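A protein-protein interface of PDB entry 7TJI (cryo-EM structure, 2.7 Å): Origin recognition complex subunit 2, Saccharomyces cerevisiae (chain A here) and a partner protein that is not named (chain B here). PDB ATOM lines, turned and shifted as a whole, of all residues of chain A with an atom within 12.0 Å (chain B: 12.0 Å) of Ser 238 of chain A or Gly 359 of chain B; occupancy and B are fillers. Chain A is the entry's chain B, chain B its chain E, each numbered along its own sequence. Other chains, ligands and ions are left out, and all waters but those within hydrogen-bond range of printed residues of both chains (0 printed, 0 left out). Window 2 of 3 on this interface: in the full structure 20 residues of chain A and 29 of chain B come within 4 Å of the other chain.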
ATOM      1  N   ALA A 236      12.127  -0.586  -9.757  1.00  0.00           N
ATOM      2  CA  ALA A 236      10.937   0.201 -10.057  1.00  0.00           C
ATOM      3  C   ALA A 236       9.803  -0.691 -10.551  1.00  0.00           C
ATOM      4  O   ALA A 236       8.875  -0.221 -11.207  1.00  0.00           O
ATOM      5  CB  ALA A 236      11.255   1.271 -11.085  1.00  0.00           C
ATOM      6  N   SER A 237       9.883  -1.980 -10.232  1.00  0.00           N
ATOM      7  CA  SER A 237       8.890  -2.947 -10.672  1.00  0.00           C
ATOM      8  C   SER A 237       8.527  -3.861  -9.514  1.00  0.00           C
ATOM      9  O   SER A 237       9.414  -4.419  -8.863  1.00  0.00           O
ATOM     10  CB  SER A 237       9.414  -3.772 -11.853  1.00  0.00           C
ATOM     11  OG  SER A 237       8.497  -4.792 -12.209  1.00  0.00           O
ATOM     12  N   SER A 238       7.223  -4.004  -9.257  1.00  0.00           N
ATOM     13  CA  SER A 238       6.762  -4.922  -8.219  1.00  0.00           C
ATOM     14  C   SER A 238       7.034  -6.372  -8.602  1.00  0.00           C
ATOM     15  O   SER A 238       7.421  -7.183  -7.754  1.00  0.00           O
ATOM     16  CB  SER A 238       5.271  -4.710  -7.952  1.00  0.00           C
ATOM     17  OG  SER A 238       5.028  -3.433  -7.393  1.00  0.00           O
ATOM     18  N   PHE A 239       6.837  -6.713  -9.869  1.00  0.00           N
ATOM     19  CA  PHE A 239       7.132  -8.039 -10.383  1.00  0.00           C
ATOM     20  C   PHE A 239       8.466  -8.013 -11.113  1.00  0.00           C
ATOM     21  O   PHE A 239       8.763  -7.069 -11.849  1.00  0.00           O
ATOM     22  CB  PHE A 239       6.031  -8.522 -11.325  1.00  0.00           C
ATOM     23  CG  PHE A 239       4.649  -8.211 -10.847  1.00  0.00           C
ATOM     24  CD1 PHE A 239       4.174  -8.760  -9.665  1.00  0.00           C
ATOM     25  CD2 PHE A 239       3.823  -7.365 -11.572  1.00  0.00           C
ATOM     26  CE1 PHE A 239       2.899  -8.480  -9.220  1.00  0.00           C
ATOM     27  CE2 PHE A 239       2.545  -7.082 -11.133  1.00  0.00           C
ATOM     28  CZ  PHE A 239       2.083  -7.643  -9.957  1.00  0.00           C
ATOM     29  N   LEU A 240       9.269  -9.051 -10.903  1.00  0.00           N
ATOM     30  CA  LEU A 240      10.582  -9.131 -11.522  1.00  0.00           C
ATOM     31  C   LEU A 240      10.640 -10.203 -12.599  1.00  0.00           C
ATOM     32  O   LEU A 240      10.941  -9.898 -13.756  1.00  0.00           O
ATOM     33  CB  LEU A 240      11.661  -9.395 -10.463  1.00  0.00           C
ATOM     34  CG  LEU A 240      12.365  -8.167  -9.887  1.00  0.00           C
ATOM     35  CD1 LEU A 240      13.357  -8.574  -8.808  1.00  0.00           C
ATOM     36  CD2 LEU A 240      13.065  -7.405 -10.994  1.00  0.00           C
ATOM     37  N   ASP A 241      10.349 -11.459 -12.256  1.00  0.00           N
ATOM     38  CA  ASP A 241      10.604 -12.541 -13.199  1.00  0.00           C
ATOM     39  C   ASP A 241       9.451 -13.547 -13.236  1.00  0.00           C
ATOM     40  O   ASP A 241       9.557 -14.652 -12.699  1.00  0.00           O
ATOM     41  CB  ASP A 241      11.924 -13.212 -12.838  1.00  0.00           C
ATOM     42  CG  ASP A 241      12.075 -13.458 -11.354  1.00  0.00           C
ATOM     43  OD1 ASP A 241      11.114 -13.199 -10.605  1.00  0.00           O
ATOM     44  OD2 ASP A 241      13.156 -13.916 -10.934  1.00  0.00           O
ATOM     45  N   THR A 242       8.396 -13.183 -13.956  1.00  0.00           N
ATOM     46  CA  THR A 242       7.277 -14.023 -14.404  1.00  0.00           C
ATOM     47  C   THR A 242       6.807 -13.430 -15.728  1.00  0.00           C
ATOM     48  O   THR A 242       7.543 -12.679 -16.376  1.00  0.00           O
ATOM     49  CB  THR A 242       6.097 -14.092 -13.403  1.00  0.00           C
ATOM     50  OG1 THR A 242       5.458 -12.815 -13.326  1.00  0.00           O
ATOM     51  CG2 THR A 242       6.439 -14.615 -11.998  1.00  0.00           C
ATOM     52  N   PHE A 243       5.577 -13.755 -16.138  1.00  0.00           N
ATOM     53  CA  PHE A 243       4.972 -12.995 -17.230  1.00  0.00           C
ATOM     54  C   PHE A 243       4.576 -11.600 -16.750  1.00  0.00           C
ATOM     55  O   PHE A 243       4.574 -10.641 -17.537  1.00  0.00           O
ATOM     56  CB  PHE A 243       3.817 -13.816 -17.864  1.00  0.00           C
ATOM     57  CG  PHE A 243       2.617 -14.144 -16.948  1.00  0.00           C
ATOM     58  CD1 PHE A 243       1.755 -13.168 -16.439  1.00  0.00           C
ATOM     59  CD2 PHE A 243       2.397 -15.456 -16.559  1.00  0.00           C
ATOM     60  CE1 PHE A 243       0.692 -13.507 -15.627  1.00  0.00           C
ATOM     61  CE2 PHE A 243       1.344 -15.795 -15.729  1.00  0.00           C
ATOM     62  CZ  PHE A 243       0.495 -14.819 -15.266  1.00  0.00           C
ATOM     63  N   GLU A 244       4.273 -11.478 -15.450  1.00  0.00           N
ATOM     64  CA  GLU A 244       3.916 -10.192 -14.864  1.00  0.00           C
ATOM     65  C   GLU A 244       5.105  -9.250 -14.858  1.00  0.00           C
ATOM     66  O   GLU A 244       4.940  -8.050 -15.077  1.00  0.00           O
ATOM     67  CB  GLU A 244       3.393 -10.373 -13.440  1.00  0.00           C
ATOM     68  CG  GLU A 244       2.364 -11.455 -13.271  1.00  0.00           C
ATOM     69  CD  GLU A 244       0.984 -10.907 -12.988  1.00  0.00           C
ATOM     70  OE1 GLU A 244       0.868  -9.688 -12.749  1.00  0.00           O
ATOM     71  OE2 GLU A 244       0.016 -11.695 -13.005  1.00  0.00           O
ATOM     72  N   GLY A 245       6.305  -9.775 -14.598  1.00  0.00           N
ATOM     73  CA  GLY A 245       7.506  -8.961 -14.689  1.00  0.00           C
ATOM     74  C   GLY A 245       7.797  -8.493 -16.098  1.00  0.00           C
ATOM     75  O   GLY A 245       8.293  -7.378 -16.293  1.00  0.00           O
ATOM     76  N   TYR A 246       7.486  -9.331 -17.093  1.00  0.00           N
ATOM     77  CA  TYR A 246       7.615  -8.932 -18.489  1.00  0.00           C
ATOM     78  C   TYR A 246       6.682  -7.778 -18.822  1.00  0.00           C
ATOM     79  O   TYR A 246       7.104  -6.782 -19.418  1.00  0.00           O
ATOM     80  CB  TYR A 246       7.329 -10.112 -19.413  1.00  0.00           C
ATOM     81  CG  TYR A 246       7.353  -9.730 -20.875  1.00  0.00           C
ATOM     82  CD1 TYR A 246       8.548  -9.427 -21.504  1.00  0.00           C
ATOM     83  CD2 TYR A 246       6.181  -9.662 -21.623  1.00  0.00           C
ATOM     84  CE1 TYR A 246       8.586  -9.078 -22.840  1.00  0.00           C
ATOM     85  CE2 TYR A 246       6.206  -9.307 -22.963  1.00  0.00           C
ATOM     86  CZ  TYR A 246       7.413  -9.021 -23.564  1.00  0.00           C
ATOM     87  OH  TYR A 246       7.460  -8.664 -24.887  1.00  0.00           O
ATOM     88  N   PHE A 247       5.404  -7.896 -18.443  1.00  0.00           N
ATOM     89  CA  PHE A 247       4.475  -6.802 -18.722  1.00  0.00           C
ATOM     90  C   PHE A 247       4.781  -5.570 -17.875  1.00  0.00           C
ATOM     91  O   PHE A 247       4.564  -4.441 -18.328  1.00  0.00           O
ATOM     92  CB  PHE A 247       3.032  -7.253 -18.500  1.00  0.00           C
ATOM     93  CG  PHE A 247       2.632  -8.441 -19.322  1.00  0.00           C
ATOM     94  CD1 PHE A 247       2.985  -8.528 -20.659  1.00  0.00           C
ATOM     95  CD2 PHE A 247       1.888  -9.467 -18.761  1.00  0.00           C
ATOM     96  CE1 PHE A 247       2.614  -9.626 -21.419  1.00  0.00           C
ATOM     97  CE2 PHE A 247       1.515 -10.567 -19.514  1.00  0.00           C
ATOM     98  CZ  PHE A 247       1.879 -10.644 -20.847  1.00  0.00           C
ATOM     99  N   ASP A 248       5.311  -5.764 -16.668  1.00  0.00           N
ATOM    100  CA  ASP A 248       5.570  -4.666 -15.747  1.00  0.00           C
ATOM    101  C   ASP A 248       6.778  -3.840 -16.165  1.00  0.00           C
ATOM    102  O   ASP A 248       6.760  -2.612 -16.040  1.00  0.00           O
ATOM    103  CB  ASP A 248       5.764  -5.219 -14.334  1.00  0.00           C
ATOM    104  CG  ASP A 248       5.509  -4.181 -13.258  1.00  0.00           C
ATOM    105  OD1 ASP A 248       6.349  -3.270 -13.094  1.00  0.00           O
ATOM    106  OD2 ASP A 248       4.467  -4.275 -12.576  1.00  0.00           O
ATOM    107  N   GLN A 249       7.836  -4.480 -16.660  1.00  0.00           N
ATOM    108  CA  GLN A 249       9.025  -3.709 -16.989  1.00  0.00           C
ATOM    109  C   GLN A 249       8.945  -3.028 -18.346  1.00  0.00           C
ATOM    110  O   GLN A 249       9.845  -2.246 -18.675  1.00  0.00           O
ATOM    111  CB  GLN A 249      10.269  -4.592 -16.919  1.00  0.00           C
ATOM    112  CG  GLN A 249      10.912  -4.613 -15.538  1.00  0.00           C
ATOM    113  CD  GLN A 249      11.484  -5.968 -15.189  1.00  0.00           C
ATOM    114  OE1 GLN A 249      11.202  -6.960 -15.858  1.00  0.00           O
ATOM    115  NE2 GLN A 249      12.285  -6.021 -14.127  1.00  0.00           N
ATOM    116  N   ARG A 250       7.912  -3.295 -19.139  1.00  0.00           N
ATOM    117  CA  ARG A 250       7.665  -2.537 -20.366  1.00  0.00           C
ATOM    118  C   ARG A 250       6.640  -1.431 -20.123  1.00  0.00           C
ATOM    119  O   ARG A 250       5.592  -1.361 -20.762  1.00  0.00           O
ATOM    120  CB  ARG A 250       7.211  -3.465 -21.485  1.00  0.00           C
ATOM    121  CG  ARG A 250       8.105  -4.656 -21.704  1.00  0.00           C
ATOM    122  CD  ARG A 250       7.391  -5.691 -22.538  1.00  0.00           C
ATOM    123  NE  ARG A 250       7.336  -5.311 -23.943  1.00  0.00           N
ATOM    124  CZ  ARG A 250       8.276  -5.598 -24.832  1.00  0.00           C
ATOM    125  NH1 ARG A 250       9.353  -6.288 -24.497  1.00  0.00           N
ATOM    126  NH2 ARG A 250       8.134  -5.181 -26.086  1.00  0.00           N
ATOM    127  N   LYS A 251       6.958  -0.555 -19.178  1.00  0.00           N
ATOM    128  CA  LYS A 251       6.148   0.631 -18.960  1.00  0.00           C
ATOM    129  C   LYS A 251       6.585   1.736 -19.919  1.00  0.00           C
ATOM    130  O   LYS A 251       7.465   1.555 -20.764  1.00  0.00           O
ATOM    131  CB  LYS A 251       6.246   1.088 -17.507  1.00  0.00           C
ATOM    132  CG  LYS A 251       5.327   0.340 -16.561  1.00  0.00           C
ATOM    133  CD  LYS A 251       5.789   0.481 -15.119  1.00  0.00           C
ATOM    134  CE  LYS A 251       4.920  -0.333 -14.171  1.00  0.00           C
ATOM    135  NZ  LYS A 251       4.354  -1.545 -14.822  1.00  0.00           N
ATOM    136  N   ALA B 347      -0.728  -5.756 -19.804  1.00  0.00           N
ATOM    137  CA  ALA B 347      -0.744  -5.767 -18.345  1.00  0.00           C
ATOM    138  C   ALA B 347      -2.108  -5.430 -17.758  1.00  0.00           C
ATOM    139  O   ALA B 347      -2.285  -5.568 -16.544  1.00  0.00           O
ATOM    140  CB  ALA B 347       0.301  -4.795 -17.798  1.00  0.00           C
ATOM    141  N   SER B 348      -3.062  -4.982 -18.570  1.00  0.00           N
ATOM    142  CA  SER B 348      -4.412  -4.719 -18.098  1.00  0.00           C
ATOM    143  C   SER B 348      -5.307  -5.947 -18.092  1.00  0.00           C
ATOM    144  O   SER B 348      -6.404  -5.887 -17.529  1.00  0.00           O
ATOM    145  CB  SER B 348      -5.074  -3.642 -18.954  1.00  0.00           C
ATOM    146  OG  SER B 348      -6.420  -3.462 -18.554  1.00  0.00           O
ATOM    147  N   SER B 351      -2.605  -9.719 -15.914  1.00  0.00           N
ATOM    148  CA  SER B 351      -1.883  -9.490 -14.667  1.00  0.00           C
ATOM    149  C   SER B 351      -2.800  -9.752 -13.478  1.00  0.00           C
ATOM    150  O   SER B 351      -3.787  -9.037 -13.280  1.00  0.00           O
ATOM    151  CB  SER B 351      -1.333  -8.069 -14.622  1.00  0.00           C
ATOM    152  OG  SER B 351      -0.068  -7.998 -15.253  1.00  0.00           O
ATOM    153  N   ARG B 352      -2.460 -10.769 -12.676  1.00  0.00           N
ATOM    154  CA  ARG B 352      -3.321 -11.177 -11.572  1.00  0.00           C
ATOM    155  C   ARG B 352      -2.552 -11.483 -10.289  1.00  0.00           C
ATOM    156  O   ARG B 352      -3.140 -12.019  -9.343  1.00  0.00           O
ATOM    157  CB  ARG B 352      -4.142 -12.408 -11.962  1.00  0.00           C
ATOM    158  CG  ARG B 352      -3.301 -13.641 -12.256  1.00  0.00           C
ATOM    159  CD  ARG B 352      -4.133 -14.720 -12.922  1.00  0.00           C
ATOM    160  NE  ARG B 352      -3.532 -15.209 -14.155  1.00  0.00           N
ATOM    161  CZ  ARG B 352      -2.689 -16.230 -14.222  1.00  0.00           C
ATOM    162  NH1 ARG B 352      -2.293 -16.872 -13.136  1.00  0.00           N
ATOM    163  NH2 ARG B 352      -2.235 -16.620 -15.410  1.00  0.00           N
ATOM    164  N   LYS B 353      -1.267 -11.161 -10.219  1.00  0.00           N
ATOM    165  CA  LYS B 353      -0.470 -11.467  -9.042  1.00  0.00           C
ATOM    166  C   LYS B 353      -0.455 -10.281  -8.087  1.00  0.00           C
ATOM    167  O   LYS B 353      -0.498  -9.122  -8.505  1.00  0.00           O
ATOM    168  CB  LYS B 353       0.962 -11.844  -9.427  1.00  0.00           C
ATOM    169  CG  LYS B 353       1.091 -13.163 -10.187  1.00  0.00           C
ATOM    170  CD  LYS B 353       0.237 -14.269  -9.584  1.00  0.00           C
ATOM    171  CE  LYS B 353       0.485 -15.598 -10.276  1.00  0.00           C
ATOM    172  NZ  LYS B 353       0.450 -15.469 -11.759  1.00  0.00           N
ATOM    173  N   THR B 354      -0.399 -10.587  -6.793  1.00  0.00           N
ATOM    174  CA  THR B 354      -0.362  -9.547  -5.779  1.00  0.00           C
ATOM    175  C   THR B 354       1.034  -8.939  -5.688  1.00  0.00           C
ATOM    176  O   THR B 354       2.003  -9.451  -6.253  1.00  0.00           O
ATOM    177  CB  THR B 354      -0.795 -10.103  -4.421  1.00  0.00           C
ATOM    178  OG1 THR B 354      -0.241 -11.409  -4.236  1.00  0.00           O
ATOM    179  CG2 THR B 354      -2.312 -10.188  -4.341  1.00  0.00           C
ATOM    180  N   ARG B 355       1.128  -7.832  -4.956  1.00  0.00           N
ATOM    181  CA  ARG B 355       2.322  -6.998  -4.944  1.00  0.00           C
ATOM    182  C   ARG B 355       2.850  -6.815  -3.530  1.00  0.00           C
ATOM    183  O   ARG B 355       2.078  -6.710  -2.572  1.00  0.00           O
ATOM    184  CB  ARG B 355       2.039  -5.621  -5.551  1.00  0.00           C
ATOM    185  CG  ARG B 355       1.707  -5.640  -7.022  1.00  0.00           C
ATOM    186  CD  ARG B 355       1.008  -4.362  -7.437  1.00  0.00           C
ATOM    187  NE  ARG B 355       0.489  -4.440  -8.797  1.00  0.00           N
ATOM    188  CZ  ARG B 355       1.088  -3.917  -9.857  1.00  0.00           C
ATOM    189  NH1 ARG B 355       2.236  -3.271  -9.750  1.00  0.00           N
ATOM    190  NH2 ARG B 355       0.522  -4.048 -11.053  1.00  0.00           N
ATOM    191  N   ILE B 356       4.173  -6.777  -3.414  1.00  0.00           N
ATOM    192  CA  ILE B 356       4.848  -6.340  -2.202  1.00  0.00           C
ATOM    193  C   ILE B 356       5.352  -4.910  -2.342  1.00  0.00           C
ATOM    194  O   ILE B 356       5.245  -4.111  -1.411  1.00  0.00           O
ATOM    195  CB  ILE B 356       5.996  -7.318  -1.859  1.00  0.00           C
ATOM    196  CG1 ILE B 356       5.438  -8.722  -1.632  1.00  0.00           C
ATOM    197  CG2 ILE B 356       6.759  -6.880  -0.614  1.00  0.00           C
ATOM    198  CD1 ILE B 356       5.863  -9.727  -2.668  1.00  0.00           C
ATOM    199  N   ILE B 357       5.859  -4.565  -3.514  1.00  0.00           N
ATOM    200  CA  ILE B 357       6.231  -3.199  -3.859  1.00  0.00           C
ATOM    201  C   ILE B 357       4.985  -2.469  -4.349  1.00  0.00           C
ATOM    202  O   ILE B 357       4.085  -3.072  -4.943  1.00  0.00           O
ATOM    203  CB  ILE B 357       7.356  -3.201  -4.915  1.00  0.00           C
ATOM    204  CG1 ILE B 357       8.405  -4.263  -4.572  1.00  0.00           C
ATOM    205  CG2 ILE B 357       8.013  -1.832  -5.044  1.00  0.00           C
ATOM    206  CD1 ILE B 357       9.194  -3.970  -3.309  1.00  0.00           C
ATOM    207  N   GLN B 358       4.914  -1.166  -4.072  1.00  0.00           N
ATOM    208  CA  GLN B 358       3.809  -0.349  -4.557  1.00  0.00           C
ATOM    209  C   GLN B 358       3.859  -0.222  -6.075  1.00  0.00           C
ATOM    210  O   GLN B 358       4.926  -0.032  -6.665  1.00  0.00           O
ATOM    211  CB  GLN B 358       3.854   1.040  -3.921  1.00  0.00           C
ATOM    212  CG  GLN B 358       4.149   1.036  -2.434  1.00  0.00           C
ATOM    213  CD  GLN B 358       3.872   2.373  -1.781  1.00  0.00           C
ATOM    214  OE1 GLN B 358       3.965   3.421  -2.420  1.00  0.00           O
ATOM    215  NE2 GLN B 358       3.531   2.346  -0.498  1.00  0.00           N
ATOM    216  N   GLY B 359       2.694  -0.333  -6.707  1.00  0.00           N
ATOM    217  CA  GLY B 359       2.621  -0.247  -8.151  1.00  0.00           C
ATOM    218  C   GLY B 359       1.214  -0.375  -8.694  1.00  0.00           C
ATOM    219  O   GLY B 359       0.329  -0.919  -8.030  1.00  0.00           O
ATOM    220  N   ARG B 360       0.998   0.127  -9.906  1.00  0.00           N
ATOM    221  CA  ARG B 360      -0.304   0.106 -10.552  1.00  0.00           C
ATOM    222  C   ARG B 360      -0.197  -0.586 -11.902  1.00  0.00           C
ATOM    223  O   ARG B 360       0.751  -0.351 -12.657  1.00  0.00           O
ATOM    224  CB  ARG B 360      -0.854   1.522 -10.751  1.00  0.00           C
ATOM    225  CG  ARG B 360      -0.759   2.417  -9.533  1.00  0.00           C
ATOM    226  CD  ARG B 360      -0.698   3.874  -9.944  1.00  0.00           C
ATOM    227  NE  ARG B 360      -2.011   4.377 -10.325  1.00  0.00           N
ATOM    228  CZ  ARG B 360      -2.600   5.427  -9.771  1.00  0.00           C
ATOM    229  NH1 ARG B 360      -2.019   6.114  -8.802  1.00  0.00           N
ATOM    230  NH2 ARG B 360      -3.803   5.795 -10.199  1.00  0.00           N
ATOM    231  N   ALA B 361      -1.177  -1.429 -12.205  1.00  0.00           N
ATOM    232  CA  ALA B 361      -1.241  -2.074 -13.505  1.00  0.00           C
ATOM    233  C   ALA B 361      -1.813  -1.108 -14.542  1.00  0.00           C
ATOM    234  O   ALA B 361      -2.207   0.021 -14.233  1.00  0.00           O
ATOM    235  CB  ALA B 361      -2.070  -3.353 -13.423  1.00  0.00           C
ATOM    236  N   ALA B 362      -1.844  -1.556 -15.793  1.00  0.00           N
ATOM    237  CA  ALA B 362      -2.433  -0.764 -16.863  1.00  0.00           C
ATOM    238  C   ALA B 362      -3.944  -0.667 -16.683  1.00  0.00           C
ATOM    239  O   ALA B 362      -4.606  -1.646 -16.326  1.00  0.00           O
ATOM    240  CB  ALA B 362      -2.099  -1.378 -18.219  1.00  0.00           C
ATOM    241  N   TYR B 363      -4.485   0.530 -16.919  1.00  0.00           N
ATOM    242  CA  TYR B 363      -5.914   0.748 -16.728  1.00  0.00           C
ATOM    243  C   TYR B 363      -6.745   0.086 -17.816  1.00  0.00           C
ATOM    244  O   TYR B 363      -7.905  -0.260 -17.568  1.00  0.00           O
ATOM    245  CB  TYR B 363      -6.246   2.243 -16.692  1.00  0.00           C
ATOM    246  CG  TYR B 363      -5.402   3.104 -15.768  1.00  0.00           C
ATOM    247  CD1 TYR B 363      -4.934   2.625 -14.545  1.00  0.00           C
ATOM    248  CD2 TYR B 363      -5.089   4.412 -16.120  1.00  0.00           C
ATOM    249  CE1 TYR B 363      -4.165   3.420 -13.713  1.00  0.00           C
ATOM    250  CE2 TYR B 363      -4.330   5.215 -15.293  1.00  0.00           C
ATOM    251  CZ  TYR B 363      -3.868   4.714 -14.094  1.00  0.00           C
ATOM    252  OH  TYR B 363      -3.110   5.517 -13.273  1.00  0.00           O
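Hydrophobic or aromatic side chains of chain B within 4 Å of the printed part of chain A: Ala 347 and Ile 357.
Along chain B the printed residues that touch a printed residue of chain A span positions 347 to 359.
Hydrophobic or aromatic side chains of chain A that line the printed part of chain B: Phe 239, Phe 243 and Phe 247.
Among the printed residues, 14 pairs touch across the chains.
Among the printed residues, Asp or Glu carboxylates within 4 Å of a Lys or Arg side-chain nitrogen of the other chain: Glu 244 of chain A with Lys 353 of chain B and Asp 248 of chain A with Arg 355 of chain B.
The backbone NH (N) of Phe 239 of chain A lies close to the side-chain hydroxyl (OG) of Ser 237 of chain A (3.5 Å).
The side-chain hydroxyl (OG) of Ser 237 of chain A is in hydrogen-bond range of the side-chain carboxylate (OD1) of Asp 248 of chain A, at 2.8 Å.
OG1 of Thr 242 of chain A is in hydrogen-bond range of N of Glu 244 of chain A (2.8 Å).
The side-chain carboxylate (OD1) of Asp 248 of chain A is in salt-bridge range of the side-chain amino group (NZ) of Lys 251 of chain A, 3.2 Å away.
NH1 of Arg 355 of chain B lies close to O of Gly 359 of chain B (3.5 Å).
Arg 355 of chain B touches Ser 238 of chain A.
OG of Ser 238 of chain A touches N of Gly 359 of chain B (3.9 Å).
CZ of Phe 239 of chain A touches O of Lys 353 of chain B, at 3.3 Å.
Phe 239 of chain A touches Thr 354 of chain B (CE1 to O, 3.2 Å).
CG of Arg 355 of chain B touches CZ of Phe 239 of chain A, at 3.6 Å.
Phe 243 of chain A touches Arg 352 of chain B.
Phe 243 of chain A touches Lys 353 of chain B.
Phe 247 of chain A touches Ala 347 of chain B.
O of Ile 357 of chain B sits at hydrogen-bond distance from OG of Ser 238 of chain A, 2.6 Å away.
The backbone carbonyl oxygen (O) of Gln 358 of chain B lies within hydrogen-bond range of the side-chain hydroxyl (OG) of Ser 238 of chain A (3.5 Å).
OE1 of Glu 244 of chain A is in hydrogen-bond range of OG of Ser 351 of chain B (3.2 Å).
OE2 of Glu 244 of chain A sits at hydrogen-bond distance from N of Arg 352 of chain B (2.7 Å).
The side-chain amino group (NZ) of Lys 353 of chain B is in salt-bridge range of the side-chain carboxylate (OE2) of Glu 244 of chain A (3.998 Å).
The guanidinium group of Arg 355 of chain B lies within salt-bridge range of the side-chain carboxylate of Asp 248 of chain A, 3.7 Å away.
No residue of chain B comes within 4 Å of Ala 236 of chain A.
Ser 238 of chain A touches just these residues of chain B: Arg 355 (3.7 Å), Ile 357 (2.6 Å), Gln 358 (3.5 Å) and Gly 359 (3.9 Å).
Phe 239 of chain A touches just these residues of chain B: Lys 353, Thr 354 and Arg 355.
Printed residues of chain B within 4 Å of Phe 243 of chain A: Arg 352 and Lys 353.
No residue of chain B comes within 4 Å of Gly 245 of chain A.
Printed residues of chain B within 4 Å of Phe 247 of chain A: Ala 347.
Asp 248 of chain A touches one residue of chain B.
Arg 355 of chain B touches just these residues of chain A: Ser 238 (3.7 Å), Phe 239 (3.6 Å) and Asp 248 (3.7 Å).
No residue of chain A comes within 4 Å of Ile 356 of chain B.
Of chain A, only Ser 238 comes within 4 Å of Gly 359 of chain B.
No residue of chain A comes within 4 Å of Ala 361 of chain B.
The nearest residue of chain B that does not touch Ser 238 of chain A is Ile 356 of chain B (5.1 Å).
The nearest residue of chain A that does not touch Gly 359 of chain B is Asp 248 of chain A (6.3 Å).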
